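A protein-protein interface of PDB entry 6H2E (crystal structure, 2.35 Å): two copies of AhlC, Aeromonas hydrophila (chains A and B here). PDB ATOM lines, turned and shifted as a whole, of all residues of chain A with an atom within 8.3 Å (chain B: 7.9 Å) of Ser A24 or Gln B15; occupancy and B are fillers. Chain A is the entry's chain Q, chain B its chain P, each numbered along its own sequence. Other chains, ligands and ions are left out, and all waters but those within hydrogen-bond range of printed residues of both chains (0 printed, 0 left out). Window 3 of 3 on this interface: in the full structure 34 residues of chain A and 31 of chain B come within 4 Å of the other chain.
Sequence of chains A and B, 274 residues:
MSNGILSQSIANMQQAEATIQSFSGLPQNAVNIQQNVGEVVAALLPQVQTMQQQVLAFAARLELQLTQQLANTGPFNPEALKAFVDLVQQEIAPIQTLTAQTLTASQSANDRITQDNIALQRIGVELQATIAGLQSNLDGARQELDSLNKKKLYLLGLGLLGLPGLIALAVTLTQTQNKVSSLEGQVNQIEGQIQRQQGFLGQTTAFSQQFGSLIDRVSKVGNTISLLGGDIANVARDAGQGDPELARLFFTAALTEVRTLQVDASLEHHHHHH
N of Ser A24 sits close to NE2 of Gln B15, at 2.9 Å.
The backbone carbonyl oxygen of Ser A22 sits close to the side-chain amide oxygen of Gln B15, at 3.0 Å.
O of Thr A19 lies within hydrogen-bond range of OG of Ser A22, 2.6 Å away.
The side-chain hydroxyl (OG1) of Thr B19 sits at hydrogen-bond distance from the backbone carbonyl oxygen (O) of Ala B16 (3.0 Å).
O of Phe A23 lies within hydrogen-bond range of NE2 of Gln A34, 2.8 Å away.
The side-chain hydroxyl (OG1) of Thr B19 lies within hydrogen-bond range of the side-chain amide oxygen (OE1) of Gln B203 (2.7 Å).
Among the printed residues, merely in contact across the chains: Ser A22 with Thr B19 (2.8 Å), Phe A23 with Gln B15 (3.7 Å), Phe A23 with Thr B19 (3.8 Å), Arg A196 with Gln B15 (3.9 Å) and Arg A196 with Asn B12 (3.95 Å).
Ser A24 touches one residue of chain B.
No residue of chain B comes within 4 Å of Gly A25.
Printed residues of chain B within 4 Å of Arg A196: Asn B12 (3.95 Å) and Gln B15 (3.9 Å).
Ile B10 touches none of the printed residues of chain A.
Printed residues of chain A within 4 Å of Asn B12: Arg A196.
Gln B15 touches just these residues of chain A: Ser A22 (3.0 Å), Phe A23 (3.7 Å), Ser A24 (2.9 Å) and Arg A196 (3.9 Å).
Ala B16 touches none of the printed residues of chain A.
Ala B18 touches none of the printed residues of chain A.
The nearest residue of chain B that does not touch Ser A24 is Thr B19 (6.3 Å).
Of the 17 printed residues of chain B, 3 touch a printed residue of chain A.
Hydrophobic or aromatic side chains of chain A within 4 Å of the printed part of chain B: Phe A23.
Among the printed residues, 7 pairs touch across the chains.
Positions printed for both chains: 19, 20 and 21.
Of the 7 pairs that touch across the chains among the printed residues, none has its exchanged pair printed and touching as well.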
ATOM      1  N   THR A  19      20.730  23.001 -26.299  1.00  0.00           N
ATOM      2  CA  THR A  19      20.719  21.788 -25.559  1.00  0.00           C
ATOM      3  C   THR A  19      20.430  20.579 -26.463  1.00  0.00           C
ATOM      4  O   THR A  19      20.957  19.513 -26.232  1.00  0.00           O
ATOM      5  CB  THR A  19      19.640  21.855 -24.479  1.00  0.00           C
ATOM      6  OG1 THR A  19      20.046  22.843 -23.539  1.00  0.00           O
ATOM      7  CG2 THR A  19      19.444  20.538 -23.770  1.00  0.00           C
ATOM      8  N   ILE A  20      19.531  20.742 -27.432  1.00  0.00           N
ATOM      9  CA  ILE A  20      19.240  19.683 -28.447  1.00  0.00           C
ATOM     10  C   ILE A  20      20.474  19.448 -29.332  1.00  0.00           C
ATOM     11  O   ILE A  20      20.707  18.329 -29.756  1.00  0.00           O
ATOM     12  CB  ILE A  20      17.995  20.114 -29.251  1.00  0.00           C
ATOM     13  CG1 ILE A  20      16.734  19.915 -28.410  1.00  0.00           C
ATOM     14  CG2 ILE A  20      17.887  19.426 -30.605  1.00  0.00           C
ATOM     15  CD1 ILE A  20      15.575  20.671 -28.935  1.00  0.00           C
ATOM     16  N   GLN A  21      21.257  20.501 -29.619  1.00  0.00           N
ATOM     17  CA  GLN A  21      22.429  20.327 -30.469  1.00  0.00           C
ATOM     18  C   GLN A  21      23.538  19.606 -29.708  1.00  0.00           C
ATOM     19  O   GLN A  21      24.478  19.128 -30.346  1.00  0.00           O
ATOM     20  CB  GLN A  21      23.003  21.633 -31.004  1.00  0.00           C
ATOM     21  CG  GLN A  21      22.060  22.427 -31.899  1.00  0.00           C
ATOM     22  CD  GLN A  21      21.578  21.686 -33.120  1.00  0.00           C
ATOM     23  OE1 GLN A  21      22.205  20.710 -33.572  1.00  0.00           O
ATOM     24  NE2 GLN A  21      20.450  22.172 -33.644  1.00  0.00           N
ATOM     25  N   SER A  22      23.415  19.490 -28.374  1.00  0.00           N
ATOM     26  CA  SER A  22      24.499  18.985 -27.560  1.00  0.00           C
ATOM     27  C   SER A  22      24.554  17.465 -27.617  1.00  0.00           C
ATOM     28  O   SER A  22      25.459  16.883 -27.060  1.00  0.00           O
ATOM     29  CB  SER A  22      24.396  19.461 -26.124  1.00  0.00           C
ATOM     30  OG  SER A  22      23.303  18.856 -25.436  1.00  0.00           O
ATOM     31  N   PHE A  23      23.499  16.825 -28.109  1.00  0.00           N
ATOM     32  CA  PHE A  23      23.472  15.374 -28.103  1.00  0.00           C
ATOM     33  C   PHE A  23      24.129  14.861 -29.389  1.00  0.00           C
ATOM     34  O   PHE A  23      23.835  15.349 -30.504  1.00  0.00           O
ATOM     35  CB  PHE A  23      22.046  14.838 -28.036  1.00  0.00           C
ATOM     36  CG  PHE A  23      21.387  14.998 -26.697  1.00  0.00           C
ATOM     37  CD1 PHE A  23      20.775  16.194 -26.347  1.00  0.00           C
ATOM     38  CD2 PHE A  23      21.355  13.954 -25.795  1.00  0.00           C
ATOM     39  CE1 PHE A  23      20.211  16.363 -25.092  1.00  0.00           C
ATOM     40  CE2 PHE A  23      20.775  14.123 -24.540  1.00  0.00           C
ATOM     41  CZ  PHE A  23      20.190  15.317 -24.204  1.00  0.00           C
ATOM     42  N   SER A  24      24.995  13.865 -29.231  1.00  0.00           N
ATOM     43  CA  SER A  24      25.680  13.237 -30.363  1.00  0.00           C
ATOM     44  C   SER A  24      25.462  11.719 -30.352  1.00  0.00           C
ATOM     45  O   SER A  24      25.076  11.124 -29.335  1.00  0.00           O
ATOM     46  CB  SER A  24      27.129  13.573 -30.319  1.00  0.00           C
ATOM     47  OG  SER A  24      27.659  13.147 -29.093  1.00  0.00           O
ATOM     48  N   GLY A  25      25.693  11.109 -31.516  1.00  0.00           N
ATOM     49  CA  GLY A  25      25.670   9.673 -31.645  1.00  0.00           C
ATOM     50  C   GLY A  25      24.256   9.140 -31.614  1.00  0.00           C
ATOM     51  O   GLY A  25      23.992   8.036 -31.118  1.00  0.00           O
ATOM     52  N   LEU A  26      23.333   9.900 -32.204  1.00  0.00           N
ATOM     53  CA  LEU A  26      21.955   9.470 -32.160  1.00  0.00           C
ATOM     54  C   LEU A  26      21.508   9.071 -33.559  1.00  0.00           C
ATOM     55  O   LEU A  26      22.139   9.386 -34.549  1.00  0.00           O
ATOM     56  CB  LEU A  26      21.094  10.597 -31.563  1.00  0.00           C
ATOM     57  CG  LEU A  26      21.235  10.787 -30.052  1.00  0.00           C
ATOM     58  CD1 LEU A  26      20.606  12.097 -29.593  1.00  0.00           C
ATOM     59  CD2 LEU A  26      20.608   9.616 -29.301  1.00  0.00           C
ATOM     60  N   PRO A  27      20.403   8.326 -33.668  1.00  0.00           N
ATOM     61  CA  PRO A  27      19.779   8.008 -34.953  1.00  0.00           C
ATOM     62  C   PRO A  27      19.381   9.163 -35.876  1.00  0.00           C
ATOM     63  O   PRO A  27      19.323  10.317 -35.437  1.00  0.00           O
ATOM     64  CB  PRO A  27      18.462   7.380 -34.480  1.00  0.00           C
ATOM     65  CG  PRO A  27      18.869   6.635 -33.247  1.00  0.00           C
ATOM     66  CD  PRO A  27      19.794   7.602 -32.543  1.00  0.00           C
ATOM     67  N   ALA A  30      16.751  11.632 -34.877  1.00  0.00           N
ATOM     68  CA  ALA A  30      17.180  12.675 -33.964  1.00  0.00           C
ATOM     69  C   ALA A  30      17.907  13.779 -34.740  1.00  0.00           C
ATOM     70  O   ALA A  30      17.702  14.955 -34.500  1.00  0.00           O
ATOM     71  CB  ALA A  30      18.061  12.079 -32.892  1.00  0.00           C
ATOM     72  N   VAL A  31      18.790  13.397 -35.662  1.00  0.00           N
ATOM     73  CA  VAL A  31      19.476  14.384 -36.453  1.00  0.00           C
ATOM     74  C   VAL A  31      18.447  15.205 -37.241  1.00  0.00           C
ATOM     75  O   VAL A  31      18.624  16.372 -37.381  1.00  0.00           O
ATOM     76  CB  VAL A  31      20.560  13.764 -37.343  1.00  0.00           C
ATOM     77  CG1 VAL A  31      21.241  14.826 -38.203  1.00  0.00           C
ATOM     78  CG2 VAL A  31      21.598  13.014 -36.515  1.00  0.00           C
ATOM     79  N   GLN A  34      17.338  17.959 -34.895  1.00  0.00           N
ATOM     80  CA  GLN A  34      18.422  18.923 -34.682  1.00  0.00           C
ATOM     81  C   GLN A  34      18.526  19.929 -35.816  1.00  0.00           C
ATOM     82  O   GLN A  34      18.705  21.134 -35.567  1.00  0.00           O
ATOM     83  CB  GLN A  34      19.768  18.218 -34.563  1.00  0.00           C
ATOM     84  CG  GLN A  34      19.977  17.569 -33.226  1.00  0.00           C
ATOM     85  CD  GLN A  34      21.243  16.752 -33.200  1.00  0.00           C
ATOM     86  OE1 GLN A  34      21.759  16.308 -34.219  1.00  0.00           O
ATOM     87  NE2 GLN A  34      21.751  16.551 -32.010  1.00  0.00           N
ATOM     88  N   GLY A 192      22.563   2.709 -21.693  1.00  0.00           N
ATOM     89  CA  GLY A 192      23.203   3.952 -22.074  1.00  0.00           C
ATOM     90  C   GLY A 192      22.474   4.615 -23.235  1.00  0.00           C
ATOM     91  O   GLY A 192      22.132   5.798 -23.168  1.00  0.00           O
ATOM     92  N   GLN A 195      18.928   5.821 -22.248  1.00  0.00           N
ATOM     93  CA  GLN A 195      18.999   6.952 -21.338  1.00  0.00           C
ATOM     94  C   GLN A 195      19.275   8.223 -22.149  1.00  0.00           C
ATOM     95  O   GLN A 195      18.587   9.199 -21.982  1.00  0.00           O
ATOM     96  CB  GLN A 195      20.040   6.676 -20.257  1.00  0.00           C
ATOM     97  CG  GLN A 195      20.256   7.851 -19.308  1.00  0.00           C
ATOM     98  CD  GLN A 195      21.332   7.509 -18.301  1.00  0.00           C
ATOM     99  OE1 GLN A 195      21.041   7.142 -17.158  1.00  0.00           O
ATOM    100  NE2 GLN A 195      22.590   7.585 -18.729  1.00  0.00           N
ATOM    101  N   ARG A 196      20.202   8.152 -23.114  1.00  0.00           N
ATOM    102  CA  ARG A 196      20.467   9.263 -24.023  1.00  0.00           C
ATOM    103  C   ARG A 196      19.180   9.602 -24.785  1.00  0.00           C
ATOM    104  O   ARG A 196      18.824  10.743 -24.954  1.00  0.00           O
ATOM    105  CB  ARG A 196      21.614   8.955 -24.999  1.00  0.00           C
ATOM    106  CG  ARG A 196      22.992   9.478 -24.601  1.00  0.00           C
ATOM    107  CD  ARG A 196      24.083   9.155 -25.637  1.00  0.00           C
ATOM    108  NE  ARG A 196      24.594   7.783 -25.570  1.00  0.00           N
ATOM    109  CZ  ARG A 196      24.580   6.866 -26.564  1.00  0.00           C
ATOM    110  NH1 ARG A 196      23.860   7.030 -27.671  1.00  0.00           N
ATOM    111  NH2 ARG A 196      25.314   5.771 -26.431  1.00  0.00           N
ATOM    112  N   GLN A 197      18.476   8.599 -25.288  1.00  0.00           N
ATOM    113  CA  GLN A 197      17.312   8.897 -26.108  1.00  0.00           C
ATOM    114  C   GLN A 197      16.191   9.545 -25.288  1.00  0.00           C
ATOM    115  O   GLN A 197      15.441  10.382 -25.813  1.00  0.00           O
ATOM    116  CB  GLN A 197      16.838   7.645 -26.831  1.00  0.00           C
ATOM    117  CG  GLN A 197      17.590   7.503 -28.141  1.00  0.00           C
ATOM    118  CD  GLN A 197      17.644   6.109 -28.706  1.00  0.00           C
ATOM    119  OE1 GLN A 197      18.693   5.649 -29.174  1.00  0.00           O
ATOM    120  NE2 GLN A 197      16.492   5.465 -28.715  1.00  0.00           N
ATOM    121  N   PHE A 200      17.055  13.020 -24.743  1.00  0.00           N
ATOM    122  CA  PHE A 200      16.914  13.820 -25.979  1.00  0.00           C
ATOM    123  C   PHE A 200      15.430  14.035 -26.303  1.00  0.00           C
ATOM    124  O   PHE A 200      15.054  15.114 -26.715  1.00  0.00           O
ATOM    125  CB  PHE A 200      17.699  13.190 -27.135  1.00  0.00           C
ATOM    126  CG  PHE A 200      17.543  13.906 -28.453  1.00  0.00           C
ATOM    127  CD1 PHE A 200      16.515  13.577 -29.319  1.00  0.00           C
ATOM    128  CD2 PHE A 200      18.427  14.897 -28.833  1.00  0.00           C
ATOM    129  CE1 PHE A 200      16.364  14.241 -30.523  1.00  0.00           C
ATOM    130  CE2 PHE A 200      18.242  15.586 -30.022  1.00  0.00           C
ATOM    131  CZ  PHE A 200      17.243  15.221 -30.885  1.00  0.00           C
ATOM    132  N   SER B   9      30.980   3.896 -18.764  1.00  0.00           N
ATOM    133  CA  SER B   9      30.634   4.945 -17.798  1.00  0.00           C
ATOM    134  C   SER B   9      31.274   6.279 -18.246  1.00  0.00           C
ATOM    135  O   SER B   9      30.628   7.276 -18.320  1.00  0.00           O
ATOM    136  CB  SER B   9      31.023   4.517 -16.404  1.00  0.00           C
ATOM    137  OG  SER B   9      30.263   3.381 -15.970  1.00  0.00           O
ATOM    138  N   ILE B  10      32.548   6.256 -18.654  1.00  0.00           N
ATOM    139  CA  ILE B  10      33.262   7.478 -19.047  1.00  0.00           C
ATOM    140  C   ILE B  10      32.558   8.153 -20.221  1.00  0.00           C
ATOM    141  O   ILE B  10      32.197   9.330 -20.171  1.00  0.00           O
ATOM    142  CB  ILE B  10      34.736   7.122 -19.333  1.00  0.00           C
ATOM    143  CG1 ILE B  10      35.489   6.935 -18.019  1.00  0.00           C
ATOM    144  CG2 ILE B  10      35.427   8.128 -20.236  1.00  0.00           C
ATOM    145  CD1 ILE B  10      36.901   6.460 -18.195  1.00  0.00           C
ATOM    146  N   ALA B  11      32.404   7.411 -21.310  1.00  0.00           N
ATOM    147  CA  ALA B  11      31.726   7.914 -22.453  1.00  0.00           C
ATOM    148  C   ALA B  11      30.383   8.505 -22.049  1.00  0.00           C
ATOM    149  O   ALA B  11      30.018   9.593 -22.549  1.00  0.00           O
ATOM    150  CB  ALA B  11      31.534   6.844 -23.480  1.00  0.00           C
ATOM    151  N   ASN B  12      29.616   7.804 -21.202  1.00  0.00           N
ATOM    152  CA  ASN B  12      28.269   8.356 -20.976  1.00  0.00           C
ATOM    153  C   ASN B  12      28.335   9.638 -20.139  1.00  0.00           C
ATOM    154  O   ASN B  12      27.423  10.472 -20.206  1.00  0.00           O
ATOM    155  CB  ASN B  12      27.322   7.352 -20.349  1.00  0.00           C
ATOM    156  CG  ASN B  12      26.998   6.206 -21.287  1.00  0.00           C
ATOM    157  OD1 ASN B  12      26.535   6.424 -22.407  1.00  0.00           O
ATOM    158  ND2 ASN B  12      27.143   4.990 -20.794  1.00  0.00           N
ATOM    159  N   MET B  13      29.363   9.729 -19.288  1.00  0.00           N
ATOM    160  CA  MET B  13      29.605  10.881 -18.455  1.00  0.00           C
ATOM    161  C   MET B  13      29.993  12.083 -19.349  1.00  0.00           C
ATOM    162  O   MET B  13      29.428  13.147 -19.191  1.00  0.00           O
ATOM    163  CB  MET B  13      30.682  10.590 -17.413  1.00  0.00           C
ATOM    164  CG  MET B  13      30.122   9.918 -16.153  1.00  0.00           C
ATOM    165  SD  MET B  13      31.396   9.192 -15.068  1.00  0.00           S
ATOM    166  CE  MET B  13      31.797  10.657 -14.126  1.00  0.00           C
ATOM    167  N   GLN B  14      30.880  11.891 -20.332  1.00  0.00           N
ATOM    168  CA  GLN B  14      31.211  12.942 -21.301  1.00  0.00           C
ATOM    169  C   GLN B  14      29.971  13.485 -22.013  1.00  0.00           C
ATOM    170  O   GLN B  14      29.842  14.684 -22.159  1.00  0.00           O
ATOM    171  CB  GLN B  14      32.246  12.444 -22.295  1.00  0.00           C
ATOM    172  CG  GLN B  14      33.603  12.297 -21.627  1.00  0.00           C
ATOM    173  CD  GLN B  14      34.565  11.396 -22.358  1.00  0.00           C
ATOM    174  OE1 GLN B  14      34.225  10.790 -23.364  1.00  0.00           O
ATOM    175  NE2 GLN B  14      35.760  11.261 -21.804  1.00  0.00           N
ATOM    176  N   GLN B  15      29.030  12.631 -22.414  1.00  0.00           N
ATOM    177  CA  GLN B  15      27.876  13.140 -23.158  1.00  0.00           C
ATOM    178  C   GLN B  15      26.972  13.962 -22.209  1.00  0.00           C
ATOM    179  O   GLN B  15      26.544  15.079 -22.509  1.00  0.00           O
ATOM    180  CB  GLN B  15      27.123  11.973 -23.796  1.00  0.00           C
ATOM    181  CG  GLN B  15      25.708  12.351 -24.222  1.00  0.00           C
ATOM    182  CD  GLN B  15      25.721  13.278 -25.419  1.00  0.00           C
ATOM    183  OE1 GLN B  15      25.874  14.501 -25.309  1.00  0.00           O
ATOM    184  NE2 GLN B  15      25.579  12.685 -26.594  1.00  0.00           N
ATOM    185  N   ALA B  16      26.663  13.402 -21.040  1.00  0.00           N
ATOM    186  CA  ALA B  16      25.849  14.110 -20.059  1.00  0.00           C
ATOM    187  C   ALA B  16      26.472  15.489 -19.724  1.00  0.00           C
ATOM    188  O   ALA B  16      25.755  16.483 -19.712  1.00  0.00           O
ATOM    189  CB  ALA B  16      25.674  13.255 -18.842  1.00  0.00           C
ATOM    190  N   GLU B  17      27.799  15.543 -19.511  1.00  0.00           N
ATOM    191  CA  GLU B  17      28.528  16.782 -19.205  1.00  0.00           C
ATOM    192  C   GLU B  17      28.304  17.802 -20.311  1.00  0.00           C
ATOM    193  O   GLU B  17      28.074  18.950 -20.001  1.00  0.00           O
ATOM    194  CB  GLU B  17      30.033  16.606 -19.084  1.00  0.00           C
ATOM    195  CG  GLU B  17      30.748  17.843 -18.564  1.00  0.00           C
ATOM    196  CD  GLU B  17      31.466  18.748 -19.558  1.00  0.00           C
ATOM    197  OE1 GLU B  17      31.403  18.449 -20.761  1.00  0.00           O
ATOM    198  OE2 GLU B  17      32.061  19.791 -19.112  1.00  0.00           O
ATOM    199  N   ALA B  18      28.408  17.377 -21.576  1.00  0.00           N
ATOM    200  CA  ALA B  18      28.243  18.306 -22.666  1.00  0.00           C
ATOM    201  C   ALA B  18      26.827  18.916 -22.629  1.00  0.00           C
ATOM    202  O   ALA B  18      26.644  20.106 -22.846  1.00  0.00           O
ATOM    203  CB  ALA B  18      28.519  17.613 -23.977  1.00  0.00           C
ATOM    204  N   THR B  19      25.805  18.119 -22.314  1.00  0.00           N
ATOM    205  CA  THR B  19      24.442  18.662 -22.340  1.00  0.00           C
ATOM    206  C   THR B  19      24.167  19.485 -21.073  1.00  0.00           C
ATOM    207  O   THR B  19      23.382  20.434 -21.106  1.00  0.00           O
ATOM    208  CB  THR B  19      23.379  17.588 -22.574  1.00  0.00           C
ATOM    209  OG1 THR B  19      23.226  16.832 -21.377  1.00  0.00           O
ATOM    210  CG2 THR B  19      23.759  16.679 -23.720  1.00  0.00           C
ATOM    211  N   ILE B  20      24.895  19.194 -20.003  1.00  0.00           N
ATOM    212  CA  ILE B  20      24.824  19.972 -18.792  1.00  0.00           C
ATOM    213  C   ILE B  20      25.406  21.371 -19.016  1.00  0.00           C
ATOM    214  O   ILE B  20      24.785  22.342 -18.635  1.00  0.00           O
ATOM    215  CB  ILE B  20      25.506  19.231 -17.642  1.00  0.00           C
ATOM    216  CG1 ILE B  20      24.611  18.093 -17.168  1.00  0.00           C
ATOM    217  CG2 ILE B  20      25.868  20.196 -16.512  1.00  0.00           C
ATOM    218  CD1 ILE B  20      25.288  17.103 -16.200  1.00  0.00           C
ATOM    219  N   GLN B  21      26.541  21.490 -19.704  1.00  0.00           N
ATOM    220  CA  GLN B  21      27.104  22.818 -19.973  1.00  0.00           C
ATOM    221  C   GLN B  21      26.194  23.624 -20.914  1.00  0.00           C
ATOM    222  O   GLN B  21      26.210  24.851 -20.879  1.00  0.00           O
ATOM    223  CB  GLN B  21      28.529  22.724 -20.512  1.00  0.00           C
ATOM    224  CG  GLN B  21      29.521  22.034 -19.563  1.00  0.00           C
ATOM    225  CD  GLN B  21      29.621  22.638 -18.184  1.00  0.00           C
ATOM    226  OE1 GLN B  21      29.083  23.706 -17.894  1.00  0.00           O
ATOM    227  NE2 GLN B  21      30.320  21.948 -17.307  1.00  0.00           N
ATOM    228  N   VAL B  41      35.255  15.858 -15.588  1.00  0.00           N
ATOM    229  CA  VAL B  41      35.522  15.328 -16.904  1.00  0.00           C
ATOM    230  C   VAL B  41      36.898  15.753 -17.435  1.00  0.00           C
ATOM    231  O   VAL B  41      37.579  14.985 -18.158  1.00  0.00           O
ATOM    232  CB  VAL B  41      34.397  15.729 -17.861  1.00  0.00           C
ATOM    233  CG1 VAL B  41      34.757  15.412 -19.304  1.00  0.00           C
ATOM    234  CG2 VAL B  41      33.088  15.055 -17.460  1.00  0.00           C
ATOM    235  N   LEU B  45      38.366  12.017 -14.990  1.00  0.00           N
ATOM    236  CA  LEU B  45      38.193  10.948 -15.941  1.00  0.00           C
ATOM    237  C   LEU B  45      39.519  10.606 -16.626  1.00  0.00           C
ATOM    238  O   LEU B  45      39.823   9.422 -16.801  1.00  0.00           O
ATOM    239  CB  LEU B  45      37.067  11.314 -16.909  1.00  0.00           C
ATOM    240  CG  LEU B  45      35.663  11.362 -16.298  1.00  0.00           C
ATOM    241  CD1 LEU B  45      34.603  11.367 -17.400  1.00  0.00           C
ATOM    242  CD2 LEU B  45      35.435  10.216 -15.332  1.00  0.00           C
ATOM    243  N   GLN B 203      19.613  15.189 -16.684  1.00  0.00           N
ATOM    244  CA  GLN B 203      20.948  15.057 -17.068  1.00  0.00           C
ATOM    245  C   GLN B 203      21.860  14.810 -15.860  1.00  0.00           C
ATOM    246  O   GLN B 203      22.722  13.956 -15.925  1.00  0.00           O
ATOM    247  CB  GLN B 203      21.383  16.312 -17.811  1.00  0.00           C
ATOM    248  CG  GLN B 203      20.748  16.438 -19.174  1.00  0.00           C
ATOM    249  CD  GLN B 203      20.851  15.161 -19.959  1.00  0.00           C
ATOM    250  OE1 GLN B 203      21.942  14.739 -20.351  1.00  0.00           O
ATOM    251  NE2 GLN B 203      19.714  14.533 -20.182  1.00  0.00           N
ATOM    252  N   PHE B 207      24.168  11.629 -15.054  1.00  0.00           N
ATOM    253  CA  PHE B 207      25.648  11.756 -14.826  1.00  0.00           C
ATOM    254  C   PHE B 207      26.040  11.123 -13.501  1.00  0.00           C
ATOM    255  O   PHE B 207      27.004  10.312 -13.403  1.00  0.00           O
ATOM    256  CB  PHE B 207      26.052  13.233 -14.891  1.00  0.00           C
ATOM    257  CG  PHE B 207      27.527  13.489 -14.741  1.00  0.00           C
ATOM    258  CD1 PHE B 207      28.126  13.442 -13.492  1.00  0.00           C
ATOM    259  CD2 PHE B 207      28.321  13.683 -15.858  1.00  0.00           C
ATOM    260  CE1 PHE B 207      29.486  13.623 -13.360  1.00  0.00           C
ATOM    261  CE2 PHE B 207      29.670  13.924 -15.711  1.00  0.00           C
ATOM    262  CZ  PHE B 207      30.253  13.895 -14.467  1.00  0.00           C
